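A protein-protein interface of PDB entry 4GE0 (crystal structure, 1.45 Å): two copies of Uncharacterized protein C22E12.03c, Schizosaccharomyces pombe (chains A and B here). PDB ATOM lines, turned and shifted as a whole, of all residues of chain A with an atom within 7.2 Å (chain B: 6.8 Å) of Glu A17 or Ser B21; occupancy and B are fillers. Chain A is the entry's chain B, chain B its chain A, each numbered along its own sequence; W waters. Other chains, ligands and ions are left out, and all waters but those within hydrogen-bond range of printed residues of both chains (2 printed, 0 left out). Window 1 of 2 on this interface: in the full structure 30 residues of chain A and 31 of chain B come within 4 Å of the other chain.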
ATOM      1  N   GLY A  14       5.121  30.761 -19.444  1.00  0.00           N
ATOM      2  CA  GLY A  14       4.550  31.569 -18.361  1.00  0.00           C
ATOM      3  C   GLY A  14       3.096  31.988 -18.561  1.00  0.00           C
ATOM      4  O   GLY A  14       2.557  32.699 -17.703  1.00  0.00           O
ATOM      5  N   THR A  15       2.450  31.538 -19.640  1.00  0.00           N
ATOM      6  CA  THR A  15       1.019  31.747 -19.813  1.00  0.00           C
ATOM      7  C   THR A  15       0.220  30.991 -18.768  1.00  0.00           C
ATOM      8  O   THR A  15       0.509  29.815 -18.447  1.00  0.00           O
ATOM      9  CB  THR A  15       0.551  31.341 -21.211  1.00  0.00           C
ATOM     10  OG1 THR A  15       1.084  32.255 -22.172  1.00  0.00           O
ATOM     11  CG2 THR A  15      -0.950  31.371 -21.309  1.00  0.00           C
ATOM     12  N   ASP A  16      -0.775  31.665 -18.206  1.00  0.00           N
ATOM     13  CA  ASP A  16      -1.602  31.048 -17.167  1.00  0.00           C
ATOM     14  C   ASP A  16      -2.450  29.880 -17.700  1.00  0.00           C
ATOM     15  O   ASP A  16      -3.167  30.032 -18.686  1.00  0.00           O
ATOM     16  CB  ASP A  16      -2.538  32.090 -16.553  1.00  0.00           C
ATOM     17  CG  ASP A  16      -3.359  31.515 -15.430  1.00  0.00           C
ATOM     18  OD1 ASP A  16      -2.738  31.219 -14.391  1.00  0.00           O
ATOM     19  OD2 ASP A  16      -4.576  31.285 -15.652  1.00  0.00           O
ATOM     20  N   GLU A  17      -2.455  28.762 -16.973  1.00  0.00           N
ATOM     21  CA  GLU A  17      -3.187  27.565 -17.413  1.00  0.00           C
ATOM     22  C   GLU A  17      -4.692  27.796 -17.444  1.00  0.00           C
ATOM     23  O   GLU A  17      -5.384  27.305 -18.335  1.00  0.00           O
ATOM     24  CB  GLU A  17      -2.907  26.394 -16.472  1.00  0.00           C
ATOM     25  CG  GLU A  17      -1.484  25.808 -16.538  1.00  0.00           C
ATOM     26  CD  GLU A  17      -0.455  26.511 -15.652  1.00  0.00           C
ATOM     27  OE1 GLU A  17      -0.652  27.668 -15.199  1.00  0.00           O
ATOM     28  OE2 GLU A  17       0.545  25.866 -15.344  1.00  0.00           O
ATOM     29  N   ILE A  18      -5.222  28.482 -16.435  1.00  0.00           N
ATOM     30  CA  ILE A  18      -6.666  28.685 -16.347  1.00  0.00           C
ATOM     31  C   ILE A  18      -7.141  29.572 -17.495  1.00  0.00           C
ATOM     32  O   ILE A  18      -8.145  29.278 -18.165  1.00  0.00           O
ATOM     33  CB  ILE A  18      -7.062  29.279 -14.970  1.00  0.00           C
ATOM     34  CG1 ILE A  18      -6.808  28.245 -13.853  1.00  0.00           C
ATOM     35  CG2 ILE A  18      -8.530  29.714 -14.963  1.00  0.00           C
ATOM     36  CD1 ILE A  18      -6.854  28.809 -12.450  1.00  0.00           C
ATOM     37  N   GLU A  19      -6.402  30.636 -17.753  1.00  0.00           N
ATOM     38  CA  GLU A  19      -6.803  31.577 -18.788  1.00  0.00           C
ATOM     39  C   GLU A  19      -6.614  31.071 -20.201  1.00  0.00           C
ATOM     40  O   GLU A  19      -7.343  31.470 -21.104  1.00  0.00           O
ATOM     41  CB  GLU A  19      -6.088  32.897 -18.591  1.00  0.00           C
ATOM     42  CG  GLU A  19      -6.517  33.535 -17.295  1.00  0.00           C
ATOM     43  CD  GLU A  19      -5.534  34.541 -16.777  1.00  0.00           C
ATOM     44  OE1 GLU A  19      -4.629  34.977 -17.517  1.00  0.00           O
ATOM     45  OE2 GLU A  19      -5.696  34.911 -15.598  1.00  0.00           O
ATOM     46  N   PHE A  20      -5.656  30.164 -20.390  1.00  0.00           N
ATOM     47  CA  PHE A  20      -5.594  29.442 -21.646  1.00  0.00           C
ATOM     48  C   PHE A  20      -6.776  28.479 -21.800  1.00  0.00           C
ATOM     49  O   PHE A  20      -7.463  28.492 -22.831  1.00  0.00           O
ATOM     50  CB  PHE A  20      -4.272  28.675 -21.746  1.00  0.00           C
ATOM     51  CG  PHE A  20      -4.123  27.872 -23.019  1.00  0.00           C
ATOM     52  CD1 PHE A  20      -4.688  26.601 -23.137  1.00  0.00           C
ATOM     53  CD2 PHE A  20      -3.371  28.380 -24.071  1.00  0.00           C
ATOM     54  CE1 PHE A  20      -4.554  25.868 -24.343  1.00  0.00           C
ATOM     55  CE2 PHE A  20      -3.184  27.653 -25.244  1.00  0.00           C
ATOM     56  CZ  PHE A  20      -3.785  26.390 -25.377  1.00  0.00           C
ATOM     57  N   SER A  21      -7.038  27.686 -20.766  1.00  0.00           N
ATOM     58  CA  SER A  21      -7.974  26.564 -20.905  1.00  0.00           C
ATOM     59  C   SER A  21      -9.415  26.978 -21.121  1.00  0.00           C
ATOM     60  O   SER A  21     -10.173  26.261 -21.788  1.00  0.00           O
ATOM     61  CB  SER A  21      -7.862  25.620 -19.715  1.00  0.00           C
ATOM     62  OG  SER A  21      -6.604  24.970 -19.740  1.00  0.00           O
ATOM     63  N   ALA A  22      -9.820  28.108 -20.548  1.00  0.00           N
ATOM     64  CA  ALA A  22     -11.208  28.526 -20.651  1.00  0.00           C
ATOM     65  C   ALA A  22     -11.609  28.846 -22.098  1.00  0.00           C
ATOM     66  O   ALA A  22     -12.534  28.211 -22.661  1.00  0.00           O
ATOM     67  CB  ALA A  22     -11.506  29.669 -19.679  1.00  0.00           C
ATOM     68  N   PRO A  23     -10.956  29.816 -22.749  1.00  0.00           N
ATOM     69  CA  PRO A  23     -11.331  30.013 -24.149  1.00  0.00           C
ATOM     70  C   PRO A  23     -11.085  28.795 -25.027  1.00  0.00           C
ATOM     71  O   PRO A  23     -11.840  28.561 -25.975  1.00  0.00           O
ATOM     72  CB  PRO A  23     -10.475  31.215 -24.620  1.00  0.00           C
ATOM     73  CG  PRO A  23      -9.382  31.329 -23.586  1.00  0.00           C
ATOM     74  CD  PRO A  23      -9.940  30.782 -22.285  1.00  0.00           C
ATOM     75  N   LYS A  48       6.251  25.836 -21.209  1.00  0.00           N
ATOM     76  CA  LYS A  48       6.099  25.740 -19.770  1.00  0.00           C
ATOM     77  C   LYS A  48       5.184  26.825 -19.216  1.00  0.00           C
ATOM     78  O   LYS A  48       5.556  27.999 -19.155  1.00  0.00           O
ATOM     79  CB  LYS A  48       7.445  25.732 -19.060  1.00  0.00           C
ATOM     80  CG  LYS A  48       7.306  25.179 -17.679  1.00  0.00           C
ATOM     81  CD  LYS A  48       8.591  25.254 -16.918  1.00  0.00           C
ATOM     82  CE  LYS A  48       8.337  25.021 -15.435  1.00  0.00           C
ATOM     83  NZ  LYS A  48       9.551  24.535 -14.796  1.00  0.00           N
ATOM     84  N   MET A  49       3.981  26.427 -18.842  1.00  0.00           N
ATOM     85  CA  MET A  49       2.955  27.373 -18.424  1.00  0.00           C
ATOM     86  C   MET A  49       3.326  28.020 -17.091  1.00  0.00           C
ATOM     87  O   MET A  49       4.268  27.597 -16.409  1.00  0.00           O
ATOM     88  CB  MET A  49       1.603  26.645 -18.356  1.00  0.00           C
ATOM     89  CG  MET A  49       1.240  25.983 -19.715  1.00  0.00           C
ATOM     90  SD  MET A  49       0.973  27.120 -21.074  1.00  0.00           S
ATOM     91  CE  MET A  49      -0.717  27.613 -20.732  1.00  0.00           C
ATOM     92  N   SER A  50       2.561  29.054 -16.737  1.00  0.00           N
ATOM     93  CA  SER A  50       2.815  29.854 -15.520  1.00  0.00           C
ATOM     94  C   SER A  50       3.027  29.012 -14.251  1.00  0.00           C
ATOM     95  O   SER A  50       3.951  29.255 -13.454  1.00  0.00           O
ATOM     96  CB  SER A  50       1.636  30.811 -15.300  1.00  0.00           C
ATOM     97  OG  SER A  50       1.923  31.621 -14.186  1.00  0.00           O
ATOM     98  N   ARG A  51       2.128  28.043 -14.065  1.00  0.00           N
ATOM     99  CA  ARG A  51       2.133  27.178 -12.897  1.00  0.00           C
ATOM    100  C   ARG A  51       2.652  25.765 -13.230  1.00  0.00           C
ATOM    101  O   ARG A  51       2.293  24.790 -12.574  1.00  0.00           O
ATOM    102  CB  ARG A  51       0.760  27.155 -12.218  1.00  0.00           C
ATOM    103  CG  ARG A  51       0.173  28.540 -11.980  1.00  0.00           C
ATOM    104  CD  ARG A  51       0.962  29.278 -10.958  1.00  0.00           C
ATOM    105  NE  ARG A  51       0.489  30.662 -10.846  1.00  0.00           N
ATOM    106  CZ  ARG A  51       0.797  31.477  -9.835  1.00  0.00           C
ATOM    107  NH1 ARG A  51       1.513  31.046  -8.807  1.00  0.00           N
ATOM    108  NH2 ARG A  51       0.302  32.713  -9.830  1.00  0.00           N
ATOM    109  N   ASP A  52       3.539  25.704 -14.222  1.00  0.00           N
ATOM    110  CA  ASP A  52       4.457  24.580 -14.469  1.00  0.00           C
ATOM    111  C   ASP A  52       3.885  23.438 -15.314  1.00  0.00           C
ATOM    112  O   ASP A  52       4.599  22.469 -15.542  1.00  0.00           O
ATOM    113  CB  ASP A  52       5.091  24.043 -13.184  1.00  0.00           C
ATOM    114  CG  ASP A  52       5.768  25.126 -12.400  1.00  0.00           C
ATOM    115  OD1 ASP A  52       6.561  25.874 -12.992  1.00  0.00           O
ATOM    116  OD2 ASP A  52       5.509  25.233 -11.184  1.00  0.00           O
ATOM    117  N   VAL A  53       2.673  23.569 -15.825  1.00  0.00           N
ATOM    118  CA  VAL A  53       2.193  22.589 -16.809  1.00  0.00           C
ATOM    119  C   VAL A  53       3.060  22.643 -18.052  1.00  0.00           C
ATOM    120  O   VAL A  53       3.384  23.727 -18.543  1.00  0.00           O
ATOM    121  CB  VAL A  53       0.743  22.798 -17.184  1.00  0.00           C
ATOM    122  CG1 VAL A  53       0.372  21.944 -18.448  1.00  0.00           C
ATOM    123  CG2 VAL A  53      -0.167  22.392 -16.017  1.00  0.00           C
ATOM    124  N   GLU A  54       3.504  21.495 -18.539  1.00  0.00           N
ATOM    125  CA  GLU A  54       4.181  21.447 -19.823  1.00  0.00           C
ATOM    126  C   GLU A  54       3.209  20.952 -20.877  1.00  0.00           C
ATOM    127  O   GLU A  54       2.694  19.848 -20.775  1.00  0.00           O
ATOM    128  CB  GLU A  54       5.391  20.524 -19.782  1.00  0.00           C
ATOM    129  CG  GLU A  54       6.629  21.104 -19.148  1.00  0.00           C
ATOM    130  CD  GLU A  54       7.782  20.121 -19.210  1.00  0.00           C
ATOM    131  OE1 GLU A  54       7.655  19.031 -18.614  1.00  0.00           O
ATOM    132  OE2 GLU A  54       8.768  20.393 -19.918  1.00  0.00           O
ATOM    133  N   MET A  55       2.975  21.765 -21.898  1.00  0.00           N
ATOM    134  CA  MET A  55       2.026  21.404 -22.933  1.00  0.00           C
ATOM    135  C   MET A  55       2.490  21.874 -24.298  1.00  0.00           C
ATOM    136  O   MET A  55       3.318  22.791 -24.406  1.00  0.00           O
ATOM    137  CB  MET A  55       0.626  21.878 -22.598  1.00  0.00           C
ATOM    138  CG  MET A  55       0.433  23.353 -22.647  1.00  0.00           C
ATOM    139  SD  MET A  55      -1.338  23.817 -22.889  1.00  0.00           S
ATOM    140  CE  MET A  55      -0.955  25.251 -23.836  1.00  0.00           C
ATOM    141  N   GLY A  81      -3.234  35.760 -19.883  1.00  0.00           N
ATOM    142  CA  GLY A  81      -2.312  36.344 -18.901  1.00  0.00           C
ATOM    143  C   GLY A  81      -1.444  35.287 -18.246  1.00  0.00           C
ATOM    144  O   GLY A  81      -0.999  34.366 -18.909  1.00  0.00           O
ATOM    145  N   GLY A  82      -1.237  35.419 -16.935  1.00  0.00           N
ATOM    146  CA  GLY A  82      -0.039  34.894 -16.278  1.00  0.00           C
ATOM    147  C   GLY A  82       1.023  35.965 -16.356  1.00  0.00           C
ATOM    148  O   GLY A  82       1.280  36.521 -17.434  1.00  0.00           O
ATOM    149  N   LEU B   9      -3.670  15.350  -8.439  1.00  0.00           N
ATOM    150  CA  LEU B   9      -4.655  15.613  -9.464  1.00  0.00           C
ATOM    151  C   LEU B   9      -4.565  14.526 -10.520  1.00  0.00           C
ATOM    152  O   LEU B   9      -3.594  14.469 -11.293  1.00  0.00           O
ATOM    153  CB  LEU B   9      -4.402  17.015 -10.046  1.00  0.00           C
ATOM    154  CG  LEU B   9      -5.357  17.522 -11.117  1.00  0.00           C
ATOM    155  CD1 LEU B   9      -6.824  17.278 -10.875  1.00  0.00           C
ATOM    156  CD2 LEU B   9      -5.093  18.969 -11.433  1.00  0.00           C
ATOM    157  N   ASP B  16     -10.776  16.748 -19.014  1.00  0.00           N
ATOM    158  CA  ASP B  16     -11.134  18.098 -19.422  1.00  0.00           C
ATOM    159  C   ASP B  16     -10.085  19.137 -19.002  1.00  0.00           C
ATOM    160  O   ASP B  16      -9.687  19.186 -17.828  1.00  0.00           O
ATOM    161  CB  ASP B  16     -12.482  18.473 -18.832  1.00  0.00           C
ATOM    162  CG  ASP B  16     -12.905  19.857 -19.260  1.00  0.00           C
ATOM    163  OD1 ASP B  16     -13.282  19.993 -20.431  1.00  0.00           O
ATOM    164  OD2 ASP B  16     -12.784  20.799 -18.435  1.00  0.00           O
ATOM    165  N   GLU B  17      -9.690  19.981 -19.959  1.00  0.00           N
ATOM    166  CA  GLU B  17      -8.650  20.981 -19.709  1.00  0.00           C
ATOM    167  C   GLU B  17      -9.049  21.995 -18.641  1.00  0.00           C
ATOM    168  O   GLU B  17      -8.232  22.391 -17.811  1.00  0.00           O
ATOM    169  CB  GLU B  17      -8.347  21.716 -21.011  1.00  0.00           C
ATOM    170  CG  GLU B  17      -7.651  20.877 -22.117  1.00  0.00           C
ATOM    171  CD  GLU B  17      -8.593  20.127 -23.049  1.00  0.00           C
ATOM    172  OE1 GLU B  17      -9.784  19.890 -22.724  1.00  0.00           O
ATOM    173  OE2 GLU B  17      -8.132  19.828 -24.151  1.00  0.00           O
ATOM    174  N   ILE B  18     -10.297  22.465 -18.697  1.00  0.00           N
ATOM    175  CA  ILE B  18     -10.737  23.505 -17.760  1.00  0.00           C
ATOM    176  C   ILE B  18     -10.782  22.976 -16.324  1.00  0.00           C
ATOM    177  O   ILE B  18     -10.300  23.620 -15.382  1.00  0.00           O
ATOM    178  CB  ILE B  18     -12.106  24.038 -18.191  1.00  0.00           C
ATOM    179  CG1 ILE B  18     -11.984  24.860 -19.479  1.00  0.00           C
ATOM    180  CG2 ILE B  18     -12.716  24.918 -17.083  1.00  0.00           C
ATOM    181  CD1 ILE B  18     -13.314  25.135 -20.160  1.00  0.00           C
ATOM    182  N   GLU B  19     -11.266  21.745 -16.178  1.00  0.00           N
ATOM    183  CA  GLU B  19     -11.411  21.132 -14.861  1.00  0.00           C
ATOM    184  C   GLU B  19     -10.082  20.685 -14.267  1.00  0.00           C
ATOM    185  O   GLU B  19      -9.932  20.633 -13.046  1.00  0.00           O
ATOM    186  CB  GLU B  19     -12.410  19.990 -14.937  1.00  0.00           C
ATOM    187  CG  GLU B  19     -13.791  20.520 -15.255  1.00  0.00           C
ATOM    188  CD  GLU B  19     -14.704  19.475 -15.828  1.00  0.00           C
ATOM    189  OE1 GLU B  19     -14.444  18.254 -15.698  1.00  0.00           O
ATOM    190  OE2 GLU B  19     -15.757  19.894 -16.343  1.00  0.00           O
ATOM    191  N   PHE B  20      -9.115  20.380 -15.127  1.00  0.00           N
ATOM    192  CA  PHE B  20      -7.764  20.102 -14.650  1.00  0.00           C
ATOM    193  C   PHE B  20      -7.150  21.425 -14.188  1.00  0.00           C
ATOM    194  O   PHE B  20      -6.581  21.517 -13.095  1.00  0.00           O
ATOM    195  CB  PHE B  20      -6.934  19.491 -15.783  1.00  0.00           C
ATOM    196  CG  PHE B  20      -5.492  19.255 -15.420  1.00  0.00           C
ATOM    197  CD1 PHE B  20      -4.572  20.289 -15.515  1.00  0.00           C
ATOM    198  CD2 PHE B  20      -5.074  18.011 -14.923  1.00  0.00           C
ATOM    199  CE1 PHE B  20      -3.246  20.104 -15.109  1.00  0.00           C
ATOM    200  CE2 PHE B  20      -3.739  17.805 -14.573  1.00  0.00           C
ATOM    201  CZ  PHE B  20      -2.848  18.878 -14.617  1.00  0.00           C
ATOM    202  N   SER B  21      -7.263  22.457 -15.021  1.00  0.00           N
ATOM    203  CA  SER B  21      -6.463  23.669 -14.813  1.00  0.00           C
ATOM    204  C   SER B  21      -6.876  24.481 -13.599  1.00  0.00           C
ATOM    205  O   SER B  21      -6.035  25.162 -13.006  1.00  0.00           O
ATOM    206  CB  SER B  21      -6.487  24.562 -16.054  1.00  0.00           C
ATOM    207  OG  SER B  21      -5.855  23.930 -17.159  1.00  0.00           O
ATOM    208  N   ALA B  22      -8.163  24.453 -13.250  1.00  0.00           N
ATOM    209  CA  ALA B  22      -8.637  25.273 -12.116  1.00  0.00           C
ATOM    210  C   ALA B  22      -8.065  24.824 -10.751  1.00  0.00           C
ATOM    211  O   ALA B  22      -7.334  25.590 -10.100  1.00  0.00           O
ATOM    212  CB  ALA B  22     -10.157  25.371 -12.101  1.00  0.00           C
ATOM    213  N   PRO B  23      -8.261  23.547 -10.357  1.00  0.00           N
ATOM    214  CA  PRO B  23      -7.632  23.117  -9.106  1.00  0.00           C
ATOM    215  C   PRO B  23      -6.107  23.173  -9.189  1.00  0.00           C
ATOM    216  O   PRO B  23      -5.455  23.536  -8.197  1.00  0.00           O
ATOM    217  CB  PRO B  23      -8.143  21.675  -8.899  1.00  0.00           C
ATOM    218  CG  PRO B  23      -8.626  21.240 -10.276  1.00  0.00           C
ATOM    219  CD  PRO B  23      -9.141  22.501 -10.933  1.00  0.00           C
ATOM    220  N   TRP B  24      -5.543  22.893 -10.357  1.00  0.00           N
ATOM    221  CA  TRP B  24      -4.104  22.970 -10.495  1.00  0.00           C
ATOM    222  C   TRP B  24      -3.600  24.365 -10.156  1.00  0.00           C
ATOM    223  O   TRP B  24      -2.708  24.541  -9.329  1.00  0.00           O
ATOM    224  CB  TRP B  24      -3.691  22.621 -11.924  1.00  0.00           C
ATOM    225  CG  TRP B  24      -2.212  22.692 -12.127  1.00  0.00           C
ATOM    226  CD1 TRP B  24      -1.500  23.743 -12.602  1.00  0.00           C
ATOM    227  CD2 TRP B  24      -1.269  21.643 -11.871  1.00  0.00           C
ATOM    228  NE1 TRP B  24      -0.153  23.436 -12.623  1.00  0.00           N
ATOM    229  CE2 TRP B  24       0.017  22.164 -12.142  1.00  0.00           C
ATOM    230  CE3 TRP B  24      -1.386  20.337 -11.382  1.00  0.00           C
ATOM    231  CZ2 TRP B  24       1.183  21.376 -12.040  1.00  0.00           C
ATOM    232  CZ3 TRP B  24      -0.227  19.570 -11.238  1.00  0.00           C
ATOM    233  CH2 TRP B  24       1.036  20.094 -11.585  1.00  0.00           C
ATOM    234  N   GLY B  25      -4.173  25.366 -10.805  1.00  0.00           N
ATOM    235  CA  GLY B  25      -3.709  26.740 -10.627  1.00  0.00           C
ATOM    236  C   GLY B  25      -3.983  27.273  -9.226  1.00  0.00           C
ATOM    237  O   GLY B  25      -3.223  28.102  -8.709  1.00  0.00           O
ATOM    238  N   ILE B  26      -5.074  26.812  -8.626  1.00  0.00           N
ATOM    239  CA  ILE B  26      -5.423  27.255  -7.274  1.00  0.00           C
ATOM    240  C   ILE B  26      -4.445  26.697  -6.222  1.00  0.00           C
ATOM    241  O   ILE B  26      -3.948  27.460  -5.372  1.00  0.00           O
ATOM    242  CB  ILE B  26      -6.900  26.934  -6.969  1.00  0.00           C
ATOM    243  CG1 ILE B  26      -7.796  27.861  -7.795  1.00  0.00           C
ATOM    244  CG2 ILE B  26      -7.232  27.105  -5.479  1.00  0.00           C
ATOM    245  CD1 ILE B  26      -9.259  27.400  -7.860  1.00  0.00           C
ATOM    246  N   LYS B  28      -1.411  25.591  -6.805  1.00  0.00           N
ATOM    247  CA  LYS B  28      -0.130  26.216  -7.066  1.00  0.00           C
ATOM    248  C   LYS B  28      -0.031  27.611  -6.446  1.00  0.00           C
ATOM    249  O   LYS B  28       0.961  27.929  -5.788  1.00  0.00           O
ATOM    250  CB  LYS B  28       0.156  26.252  -8.565  1.00  0.00           C
ATOM    251  CG  LYS B  28       0.635  24.917  -9.115  1.00  0.00           C
ATOM    252  CD  LYS B  28       2.163  24.826  -9.022  1.00  0.00           C
ATOM    253  CE  LYS B  28       2.634  23.500  -9.538  1.00  0.00           C
ATOM    254  NZ  LYS B  28       4.121  23.435  -9.542  1.00  0.00           N
ATOM    255  N   ARG B  29      -1.084  28.416  -6.567  1.00  0.00           N
ATOM    256  CA  ARG B  29      -1.073  29.769  -5.995  1.00  0.00           C
ATOM    257  C   ARG B  29      -0.994  29.698  -4.471  1.00  0.00           C
ATOM    258  O   ARG B  29      -0.382  30.562  -3.822  1.00  0.00           O
ATOM    259  CB  ARG B  29      -2.334  30.520  -6.414  1.00  0.00           C
ATOM    260  CG  ARG B  29      -2.265  31.041  -7.829  1.00  0.00           C
ATOM    261  CD  ARG B  29      -3.646  31.456  -8.293  1.00  0.00           C
ATOM    262  NE  ARG B  29      -3.597  32.132  -9.583  1.00  0.00           N
ATOM    263  CZ  ARG B  29      -3.493  31.497 -10.742  1.00  0.00           C
ATOM    264  NH1 ARG B  29      -3.390  30.173 -10.779  1.00  0.00           N
ATOM    265  NH2 ARG B  29      -3.512  32.199 -11.862  1.00  0.00           N
ATOM    266  N   MET B  49      -5.756  15.448 -23.929  1.00  0.00           N
ATOM    267  CA  MET B  49      -6.880  15.901 -23.127  1.00  0.00           C
ATOM    268  C   MET B  49      -8.176  15.927 -23.936  1.00  0.00           C
ATOM    269  O   MET B  49      -8.180  15.707 -25.149  1.00  0.00           O
ATOM    270  CB  MET B  49      -6.570  17.290 -22.556  1.00  0.00           C
ATOM    271  CG  MET B  49      -5.262  17.362 -21.783  1.00  0.00           C
ATOM    272  SD  MET B  49      -5.255  16.520 -20.191  1.00  0.00           S
ATOM    273  CE  MET B  49      -5.993  17.762 -19.130  1.00  0.00           C
ATOM    274  N   MET B  55      -0.450  17.400 -23.153  1.00  0.00           N
ATOM    275  CA  MET B  55       0.218  17.901 -21.947  1.00  0.00           C
ATOM    276  C   MET B  55       0.928  16.733 -21.255  1.00  0.00           C
ATOM    277  O   MET B  55       0.409  15.616 -21.244  1.00  0.00           O
ATOM    278  CB  MET B  55      -0.846  18.489 -21.021  1.00  0.00           C
ATOM    279  CG  MET B  55      -0.458  18.693 -19.568  1.00  0.00           C
ATOM    280  SD  MET B  55      -1.942  19.097 -18.605  1.00  0.00           S
ATOM    281  CE  MET B  55      -2.294  17.509 -17.860  1.00  0.00           C
ATOM    282  N   ALA B 167     -15.532  24.862 -12.116  1.00  0.00           N
ATOM    283  CA  ALA B 167     -14.219  24.322 -11.759  1.00  0.00           C
ATOM    284  C   ALA B 167     -13.449  25.209 -10.780  1.00  0.00           C
ATOM    285  O   ALA B 167     -12.764  24.704  -9.908  1.00  0.00           O
ATOM    286  CB  ALA B 167     -13.396  24.060 -12.992  1.00  0.00           C
ATOM    287  N   MET B 168     -13.585  26.525 -10.905  1.00  0.00           N
ATOM    288  CA  MET B 168     -12.916  27.426  -9.978  1.00  0.00           C
ATOM    289  C   MET B 168     -13.552  27.353  -8.571  1.00  0.00           C
ATOM    290  O   MET B 168     -12.851  27.198  -7.575  1.00  0.00           O
ATOM    291  CB  MET B 168     -12.947  28.867 -10.491  1.00  0.00           C
ATOM    292  CG  MET B 168     -12.077  29.112 -11.741  1.00  0.00           C
ATOM    293  SD  MET B 168     -10.328  28.940 -11.426  1.00  0.00           S
ATOM    294  CE  MET B 168     -10.054  30.401 -10.420  1.00  0.00           C
HETATM  295  O   HOH W   1      -0.494  32.086 -13.227  1.00  0.00           O
HETATM  296  O   HOH W   2      -2.959  28.692 -13.481  1.00  0.00           O
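Water W1 lies within hydrogen-bond range of the side-chain hydroxyl of Ser A50, the side-chain carboxylate of Asp A16, the guanidinium group of Arg A51 and the guanidinium group of Arg B29.
Water W2 lies within hydrogen-bond range of OD1 of Asp A16 (2.7 Å), OE1 of Glu A17 (3.1 Å) and NH1 of Arg B29 (3.1 Å).
The side-chain amino group (NZ) of Lys B28 is in salt-bridge range of the side-chain carboxylate (OD2) of Asp A52, 2.8 Å away.
The side-chain hydroxyl of Ser A21 sits at hydrogen-bond distance from the side-chain hydroxyl of Ser B21 (2.9 Å).
The backbone carbonyl oxygen (O) of Arg A51 lies within hydrogen-bond range of the indole nitrogen (NE1) of Trp B24, 2.8 Å away.
NH2 of Arg B29 is in salt-bridge range of OD1 of Asp A16 (2.8 Å).
The backbone NH (N) of Asp A52 sits at hydrogen-bond distance from the side-chain carboxylate (OE2) of Glu A17, 3.2 Å away.
O of Gly B25 sits at hydrogen-bond distance from NH1 of Arg B29 (2.9 Å).
NZ of Lys A48 is in salt-bridge range of OD1 of Asp A52.
The backbone carbonyl oxygen of Glu B17 is in hydrogen-bond range of the side-chain hydroxyl of Ser B21 (2.9 Å).
OD2 of Asp B16 is in hydrogen-bond range of N of Ile B18.
The side-chain carboxylate (OE2) of Glu A17 sits at hydrogen-bond distance from the backbone NH (N) of Val A53, 3.2 Å away.
Glu A17 touches Ser B21, and with the chains exchanged Ser A21 touches Glu B17.
Ile A18 touches Ser B21, and with the chains exchanged Ser A21 touches Ile B18.
Ile A18 touches Ala B22, and with the chains exchanged Ala A22 touches Ile B18.
Ser B21 touches its own counterpart, Ser A21.
Positions printed for both chains: 16, 17, 18, 19, 20, 21, 22, 23, 49 and 55.
Of the 18 pairs that touch across the chains among the printed residues, 7 have their exchanged pair printed and touching as well.
Printed residues of chain B within 4 Å of Glu A17: Ser B21 (3.6 Å) and Trp B24 (3.7 Å).
Printed residues of chain A within 4 Å of Ser B21: Glu A17 (3.6 Å), Ile A18 (3.3 Å) and Ser A21 (2.9 Å).
Printed residues of chain B within 4 Å of Asp A16: Arg B29.
Of the printed residues of chain B, Ala A22 touches Ile B18 (3.9 Å).
Of the printed residues of chain A, Glu B17 touches Ser A21.
Gly A14 touches none of the printed residues of chain B.
The nearest printed residue of chain B that does not touch Glu A17 is Gly B25 (5.6 Å).
Printed residues of chain B that touch a printed residue of chain A: Glu B17, Ile B18, Phe B20, Ser B21, Ala B22, Trp B24, Lys B28, Arg B29, Met B55 and Met B168.
Along chain B the printed residues that touch a printed residue of chain A span positions 17 to 168.
Of the 20 printed residues of chain A, 9 touch a printed residue of chain B.
Hydrophobic or aromatic side chains of chain A within 4 Å of the printed part of chain B: Ile A18 and Val A53.
Among the printed residues, 18 pairs touch across the chains.
Among the printed residues, Asp or Glu carboxylates within 4 Å of a Lys or Arg side-chain nitrogen of the other chain: Asp A16 with Arg B29 and Asp A52 with Lys B28.
Glu A17 touches Trp B24.
Ile A18 touches Ala B22 (CG1 to CA, 3.9 Å).
Met B168 touches Ile A18 (SD to CD1, 3.6 Å).
Glu B17 touches Ser A21.
O of Ser A21 touches CG1 of Ile B18 (3.3 Å).
Ala A22 touches Ile B18.
Lys B28 touches Arg A51 (CE to O, 3.3 Å).
Phe B20 touches Val A53 (CE1 to CG2, 3.9 Å).
Val A53 touches Trp B24.
CG of Met B55 touches CG1 of Val A53 (3.5 Å).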
